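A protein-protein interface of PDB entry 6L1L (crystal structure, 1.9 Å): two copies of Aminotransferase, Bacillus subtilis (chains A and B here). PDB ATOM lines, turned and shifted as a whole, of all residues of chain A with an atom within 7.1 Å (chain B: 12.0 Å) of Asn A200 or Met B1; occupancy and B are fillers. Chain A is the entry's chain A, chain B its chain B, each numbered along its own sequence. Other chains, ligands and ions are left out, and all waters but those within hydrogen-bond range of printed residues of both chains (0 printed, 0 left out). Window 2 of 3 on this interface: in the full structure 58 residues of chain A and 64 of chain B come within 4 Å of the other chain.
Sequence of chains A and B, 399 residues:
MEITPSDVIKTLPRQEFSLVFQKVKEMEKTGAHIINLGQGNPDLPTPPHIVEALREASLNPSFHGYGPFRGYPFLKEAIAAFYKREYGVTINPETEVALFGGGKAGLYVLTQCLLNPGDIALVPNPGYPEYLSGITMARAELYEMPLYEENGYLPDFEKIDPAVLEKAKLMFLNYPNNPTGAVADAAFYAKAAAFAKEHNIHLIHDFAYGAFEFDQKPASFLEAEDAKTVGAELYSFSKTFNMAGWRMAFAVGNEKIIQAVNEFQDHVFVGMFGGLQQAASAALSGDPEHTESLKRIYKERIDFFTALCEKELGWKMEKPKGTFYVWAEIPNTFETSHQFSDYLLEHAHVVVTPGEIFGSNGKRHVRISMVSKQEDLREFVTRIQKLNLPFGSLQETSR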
ATOM      1  N   LEU A 165     -18.091  24.817 -20.855  1.00  0.00           N
ATOM      2  CA  LEU A 165     -18.243  23.833 -21.926  1.00  0.00           C
ATOM      3  C   LEU A 165     -17.906  24.370 -23.312  1.00  0.00           C
ATOM      4  O   LEU A 165     -17.408  23.608 -24.154  1.00  0.00           O
ATOM      5  CB  LEU A 165     -19.650  23.205 -21.925  1.00  0.00           C
ATOM      6  CG  LEU A 165     -19.778  21.945 -21.076  1.00  0.00           C
ATOM      7  CD1 LEU A 165     -19.542  22.241 -19.625  1.00  0.00           C
ATOM      8  CD2 LEU A 165     -21.136  21.310 -21.216  1.00  0.00           C
ATOM      9  N   GLU A 166     -18.161  25.659 -23.545  1.00  0.00           N
ATOM     10  CA  GLU A 166     -17.848  26.273 -24.847  1.00  0.00           C
ATOM     11  C   GLU A 166     -16.346  26.463 -24.995  1.00  0.00           C
ATOM     12  O   GLU A 166     -15.793  26.269 -26.084  1.00  0.00           O
ATOM     13  CB  GLU A 166     -18.568  27.630 -25.043  1.00  0.00           C
ATOM     14  N   LYS A 167     -15.686  26.840 -23.909  1.00  0.00           N
ATOM     15  CA  LYS A 167     -14.243  27.028 -23.922  1.00  0.00           C
ATOM     16  C   LYS A 167     -13.442  25.678 -23.787  1.00  0.00           C
ATOM     17  O   LYS A 167     -12.269  25.592 -24.177  1.00  0.00           O
ATOM     18  CB  LYS A 167     -13.867  28.016 -22.812  1.00  0.00           C
ATOM     19  N   ALA A 168     -14.091  24.652 -23.237  1.00  0.00           N
ATOM     20  CA  ALA A 168     -13.479  23.324 -23.071  1.00  0.00           C
ATOM     21  C   ALA A 168     -13.194  22.653 -24.407  1.00  0.00           C
ATOM     22  O   ALA A 168     -14.130  22.364 -25.170  1.00  0.00           O
ATOM     23  CB  ALA A 168     -14.356  22.441 -22.206  1.00  0.00           C
ATOM     24  N   LYS A 169     -11.907  22.431 -24.700  1.00  0.00           N
ATOM     25  CA  LYS A 169     -11.478  21.835 -25.984  1.00  0.00           C
ATOM     26  C   LYS A 169     -11.036  20.384 -25.907  1.00  0.00           C
ATOM     27  O   LYS A 169     -11.057  19.684 -26.921  1.00  0.00           O
ATOM     28  CB  LYS A 169     -10.327  22.625 -26.605  1.00  0.00           C
ATOM     29  N   LEU A 170     -10.603  19.948 -24.728  1.00  0.00           N
ATOM     30  CA  LEU A 170     -10.025  18.613 -24.567  1.00  0.00           C
ATOM     31  C   LEU A 170     -10.491  18.001 -23.247  1.00  0.00           C
ATOM     32  O   LEU A 170     -10.635  18.723 -22.246  1.00  0.00           O
ATOM     33  CB  LEU A 170      -8.496  18.710 -24.596  1.00  0.00           C
ATOM     34  CG  LEU A 170      -7.697  17.421 -24.386  1.00  0.00           C
ATOM     35  CD1 LEU A 170      -8.003  16.404 -25.468  1.00  0.00           C
ATOM     36  CD2 LEU A 170      -6.209  17.721 -24.387  1.00  0.00           C
ATOM     37  N   PHE A 195     -21.633  13.174 -24.959  1.00  0.00           N
ATOM     38  CA  PHE A 195     -21.386  14.446 -24.274  1.00  0.00           C
ATOM     39  C   PHE A 195     -20.336  15.305 -25.013  1.00  0.00           C
ATOM     40  O   PHE A 195     -20.520  16.534 -25.197  1.00  0.00           O
ATOM     41  CB  PHE A 195     -20.926  14.211 -22.837  1.00  0.00           C
ATOM     42  CG  PHE A 195     -20.624  15.479 -22.093  1.00  0.00           C
ATOM     43  CD1 PHE A 195     -21.643  16.166 -21.422  1.00  0.00           C
ATOM     44  CD2 PHE A 195     -19.350  16.012 -22.091  1.00  0.00           C
ATOM     45  CE1 PHE A 195     -21.377  17.339 -20.753  1.00  0.00           C
ATOM     46  CE2 PHE A 195     -19.079  17.199 -21.419  1.00  0.00           C
ATOM     47  CZ  PHE A 195     -20.096  17.859 -20.750  1.00  0.00           C
ATOM     48  N   ALA A 196     -19.240  14.655 -25.420  1.00  0.00           N
ATOM     49  CA  ALA A 196     -18.152  15.339 -26.112  1.00  0.00           C
ATOM     50  C   ALA A 196     -18.611  15.912 -27.450  1.00  0.00           C
ATOM     51  O   ALA A 196     -18.144  16.982 -27.878  1.00  0.00           O
ATOM     52  CB  ALA A 196     -16.987  14.383 -26.314  1.00  0.00           C
ATOM     53  N   LYS A 197     -19.530  15.189 -28.095  1.00  0.00           N
ATOM     54  CA  LYS A 197     -20.051  15.580 -29.413  1.00  0.00           C
ATOM     55  C   LYS A 197     -20.869  16.873 -29.332  1.00  0.00           C
ATOM     56  O   LYS A 197     -20.606  17.823 -30.071  1.00  0.00           O
ATOM     57  CB  LYS A 197     -20.913  14.474 -30.003  1.00  0.00           C
ATOM     58  CG  LYS A 197     -20.883  14.462 -31.521  1.00  0.00           C
ATOM     59  CD  LYS A 197     -21.802  13.395 -32.085  1.00  0.00           C
ATOM     60  CE  LYS A 197     -22.096  13.649 -33.554  1.00  0.00           C
ATOM     61  NZ  LYS A 197     -22.825  14.936 -33.764  1.00  0.00           N
ATOM     62  N   GLU A 198     -21.816  16.891 -28.394  1.00  0.00           N
ATOM     63  CA  GLU A 198     -22.687  18.031 -28.115  1.00  0.00           C
ATOM     64  C   GLU A 198     -21.936  19.307 -27.812  1.00  0.00           C
ATOM     65  O   GLU A 198     -22.421  20.384 -28.130  1.00  0.00           O
ATOM     66  CB  GLU A 198     -23.604  17.715 -26.922  1.00  0.00           C
ATOM     67  N   HIS A 199     -20.755  19.196 -27.199  1.00  0.00           N
ATOM     68  CA  HIS A 199     -20.032  20.362 -26.707  1.00  0.00           C
ATOM     69  C   HIS A 199     -18.715  20.639 -27.394  1.00  0.00           C
ATOM     70  O   HIS A 199     -17.942  21.485 -26.946  1.00  0.00           O
ATOM     71  CB  HIS A 199     -19.871  20.244 -25.209  1.00  0.00           C
ATOM     72  CG  HIS A 199     -21.172  20.050 -24.507  1.00  0.00           C
ATOM     73  ND1 HIS A 199     -22.141  21.034 -24.449  1.00  0.00           N
ATOM     74  CD2 HIS A 199     -21.689  18.974 -23.874  1.00  0.00           C
ATOM     75  CE1 HIS A 199     -23.192  20.576 -23.789  1.00  0.00           C
ATOM     76  NE2 HIS A 199     -22.941  19.330 -23.427  1.00  0.00           N
ATOM     77  N   ASN A 200     -18.483  19.936 -28.498  1.00  0.00           N
ATOM     78  CA  ASN A 200     -17.252  20.030 -29.258  1.00  0.00           C
ATOM     79  C   ASN A 200     -16.018  19.943 -28.369  1.00  0.00           C
ATOM     80  O   ASN A 200     -15.304  20.933 -28.181  1.00  0.00           O
ATOM     81  CB  ASN A 200     -17.235  21.328 -30.093  1.00  0.00           C
ATOM     82  CG  ASN A 200     -16.102  21.354 -31.107  1.00  0.00           C
ATOM     83  OD1 ASN A 200     -15.665  20.305 -31.608  1.00  0.00           O
ATOM     84  ND2 ASN A 200     -15.612  22.558 -31.423  1.00  0.00           N
ATOM     85  N   ILE A 201     -15.833  18.780 -27.763  1.00  0.00           N
ATOM     86  CA  ILE A 201     -14.663  18.519 -26.922  1.00  0.00           C
ATOM     87  C   ILE A 201     -13.910  17.344 -27.538  1.00  0.00           C
ATOM     88  O   ILE A 201     -14.506  16.317 -27.799  1.00  0.00           O
ATOM     89  CB  ILE A 201     -15.068  18.204 -25.466  1.00  0.00           C
ATOM     90  CG1 ILE A 201     -16.023  19.288 -24.939  1.00  0.00           C
ATOM     91  CG2 ILE A 201     -13.833  18.162 -24.555  1.00  0.00           C
ATOM     92  CD1 ILE A 201     -16.639  18.997 -23.582  1.00  0.00           C
ATOM     93  N   HIS A 202     -12.614  17.502 -27.784  1.00  0.00           N
ATOM     94  CA  HIS A 202     -11.826  16.343 -28.234  1.00  0.00           C
ATOM     95  C   HIS A 202     -11.634  15.443 -27.020  1.00  0.00           C
ATOM     96  O   HIS A 202     -11.313  15.907 -25.922  1.00  0.00           O
ATOM     97  CB  HIS A 202     -10.470  16.712 -28.803  1.00  0.00           C
ATOM     98  CG  HIS A 202     -10.490  17.810 -29.805  1.00  0.00           C
ATOM     99  ND1 HIS A 202     -10.074  19.089 -29.516  1.00  0.00           N
ATOM    100  CD2 HIS A 202     -10.804  17.807 -31.119  1.00  0.00           C
ATOM    101  CE1 HIS A 202     -10.156  19.835 -30.606  1.00  0.00           C
ATOM    102  NE2 HIS A 202     -10.599  19.081 -31.586  1.00  0.00           N
ATOM    103  N   THR A 229     -15.476   9.780 -33.894  1.00  0.00           N
ATOM    104  CA  THR A 229     -15.927  11.079 -34.319  1.00  0.00           C
ATOM    105  C   THR A 229     -15.325  12.180 -33.455  1.00  0.00           C
ATOM    106  O   THR A 229     -14.956  13.207 -33.966  1.00  0.00           O
ATOM    107  CB  THR A 229     -17.480  11.106 -34.303  1.00  0.00           C
ATOM    108  OG1 THR A 229     -17.948  10.368 -35.440  1.00  0.00           O
ATOM    109  CG2 THR A 229     -18.044  12.517 -34.334  1.00  0.00           C
ATOM    110  N   VAL A 230     -15.201  11.934 -32.162  1.00  0.00           N
ATOM    111  CA  VAL A 230     -14.797  12.945 -31.212  1.00  0.00           C
ATOM    112  C   VAL A 230     -13.362  12.783 -30.667  1.00  0.00           C
ATOM    113  O   VAL A 230     -12.889  13.647 -29.942  1.00  0.00           O
ATOM    114  CB  VAL A 230     -15.774  12.984 -30.009  1.00  0.00           C
ATOM    115  CG1 VAL A 230     -17.188  13.327 -30.468  1.00  0.00           C
ATOM    116  CG2 VAL A 230     -15.773  11.667 -29.219  1.00  0.00           C
ATOM    117  N   LYS A 256      -8.554  13.168 -38.487  1.00  0.00           N
ATOM    118  CA  LYS A 256      -8.086  14.560 -38.340  1.00  0.00           C
ATOM    119  C   LYS A 256      -7.065  14.736 -37.200  1.00  0.00           C
ATOM    120  O   LYS A 256      -6.034  15.425 -37.359  1.00  0.00           O
ATOM    121  CB  LYS A 256      -9.262  15.515 -38.079  1.00  0.00           C
ATOM    122  CG  LYS A 256     -10.398  15.417 -39.094  1.00  0.00           C
ATOM    123  CD  LYS A 256      -9.868  15.547 -40.506  1.00  0.00           C
ATOM    124  CE  LYS A 256     -10.934  16.077 -41.455  1.00  0.00           C
ATOM    125  NZ  LYS A 256     -10.251  16.637 -42.664  1.00  0.00           N
ATOM    126  N   MET B   1     -16.549  18.815 -35.366  1.00  0.00           N
ATOM    127  CA  MET B   1     -15.528  19.691 -36.028  1.00  0.00           C
ATOM    128  C   MET B   1     -14.175  19.599 -35.332  1.00  0.00           C
ATOM    129  O   MET B   1     -13.909  20.309 -34.366  1.00  0.00           O
ATOM    130  CB  MET B   1     -15.996  21.159 -36.058  1.00  0.00           C
ATOM    131  N   GLU B   2     -13.324  18.712 -35.832  1.00  0.00           N
ATOM    132  CA  GLU B   2     -11.986  18.544 -35.261  1.00  0.00           C
ATOM    133  C   GLU B   2     -11.142  19.773 -35.571  1.00  0.00           C
ATOM    134  O   GLU B   2     -11.044  20.185 -36.714  1.00  0.00           O
ATOM    135  CB  GLU B   2     -11.299  17.306 -35.790  1.00  0.00           C
ATOM    136  CG  GLU B   2     -12.100  16.034 -35.617  1.00  0.00           C
ATOM    137  CD  GLU B   2     -12.128  15.558 -34.194  1.00  0.00           C
ATOM    138  OE1 GLU B   2     -11.708  14.412 -33.939  1.00  0.00           O
ATOM    139  OE2 GLU B   2     -12.571  16.309 -33.313  1.00  0.00           O
ATOM    140  N   ILE B   3     -10.565  20.353 -34.524  1.00  0.00           N
ATOM    141  CA  ILE B   3      -9.915  21.655 -34.577  1.00  0.00           C
ATOM    142  C   ILE B   3      -8.469  21.550 -34.120  1.00  0.00           C
ATOM    143  O   ILE B   3      -8.169  21.556 -32.930  1.00  0.00           O
ATOM    144  CB  ILE B   3     -10.665  22.719 -33.722  1.00  0.00           C
ATOM    145  CG1 ILE B   3     -12.070  22.982 -34.289  1.00  0.00           C
ATOM    146  CG2 ILE B   3      -9.890  24.027 -33.689  1.00  0.00           C
ATOM    147  CD1 ILE B   3     -12.123  23.633 -35.677  1.00  0.00           C
ATOM    148  N   THR B   4      -7.568  21.496 -35.087  1.00  0.00           N
ATOM    149  CA  THR B   4      -6.154  21.467 -34.768  1.00  0.00           C
ATOM    150  C   THR B   4      -5.699  22.707 -34.013  1.00  0.00           C
ATOM    151  O   THR B   4      -6.282  23.769 -34.183  1.00  0.00           O
ATOM    152  CB  THR B   4      -5.328  21.359 -36.035  1.00  0.00           C
ATOM    153  OG1 THR B   4      -6.086  20.706 -37.061  1.00  0.00           O
ATOM    154  CG2 THR B   4      -4.117  20.581 -35.742  1.00  0.00           C
ATOM    155  N   PRO B   5      -4.651  22.573 -33.169  1.00  0.00           N
ATOM    156  CA  PRO B   5      -4.100  23.762 -32.507  1.00  0.00           C
ATOM    157  C   PRO B   5      -3.567  24.770 -33.514  1.00  0.00           C
ATOM    158  O   PRO B   5      -3.176  24.380 -34.614  1.00  0.00           O
ATOM    159  CB  PRO B   5      -2.917  23.208 -31.674  1.00  0.00           C
ATOM    160  N   SER B   6      -3.477  26.037 -33.113  1.00  0.00           N
ATOM    161  CA  SER B   6      -2.866  27.083 -33.960  1.00  0.00           C
ATOM    162  C   SER B   6      -1.360  26.839 -34.211  1.00  0.00           C
ATOM    163  O   SER B   6      -0.784  27.304 -35.205  1.00  0.00           O
ATOM    164  CB  SER B   6      -3.113  28.481 -33.366  1.00  0.00           C
ATOM    165  OG  SER B   6      -4.512  28.786 -33.374  1.00  0.00           O
ATOM    166  N   ILE B   9      -1.462  24.449 -37.527  1.00  0.00           N
ATOM    167  CA  ILE B   9      -1.805  25.226 -38.739  1.00  0.00           C
ATOM    168  C   ILE B   9      -0.799  26.335 -39.092  1.00  0.00           C
ATOM    169  O   ILE B   9      -0.725  26.742 -40.235  1.00  0.00           O
ATOM    170  CB  ILE B   9      -3.251  25.750 -38.727  1.00  0.00           C
ATOM    171  CG1 ILE B   9      -3.539  26.530 -37.466  1.00  0.00           C
ATOM    172  CG2 ILE B   9      -4.232  24.587 -38.899  1.00  0.00           C
ATOM    173  CD1 ILE B   9      -5.013  26.802 -37.236  1.00  0.00           C
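The backbone NH (N) of Ile B3 lies within hydrogen-bond range of a ring nitrogen (NE2) of His A202, 3.2 Å away. The side-chain carboxylate of Glu B2 lies close to the backbone carbonyl oxygen of Thr A229 (3.5 Å). The side-chain amide oxygen of Asn A200 sits close to the backbone carbonyl oxygen of Met B1, at 3.3 Å.
Glu B2 touches His A202. Lys A256 touches Glu B2.
No position is printed for both chains. Of the 5 pairs that touch across the chains among the printed residues, none has its exchanged pair printed and touching as well.
Asn A200 touches one residue of chain B. Met B1 touches just one residue of chain A: Asn A200 (3.3 Å). No residue of chain B comes within 4 Å of Lys A169. No residue of chain B comes within 4 Å of Ala A196. No residue of chain B comes within 4 Å of Glu A198. No residue of chain B comes within 4 Å of His A199. Of chain B, only Glu B2 and Ile B3 come within 4 Å of His A202. Of the printed residues of chain B, Lys A256 touches Glu B2. Of the printed residues of chain A, Ile B3 touches His A202. Of the printed residues of chain A, Glu B2 touches His A202 (3.2 Å), Thr A229 (3.5 Å) and Lys A256 (3.5 Å). Of the printed residues of chain B, Thr A229 touches Glu B2. Lys A167 touches none of the printed residues of chain B. Leu A170 touches none of the printed residues of chain B.
N of His A202 is in hydrogen-bond range of O of Lys A169 (2.8 Å).
Of the 17 printed residues of chain A, 4 touch a printed residue of chain B. Among the printed residues, 5 pairs touch across the chains. Among the printed residues, no Asp or Glu carboxylate lies within 4 Å of a Lys or Arg side-chain nitrogen of the other chain.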
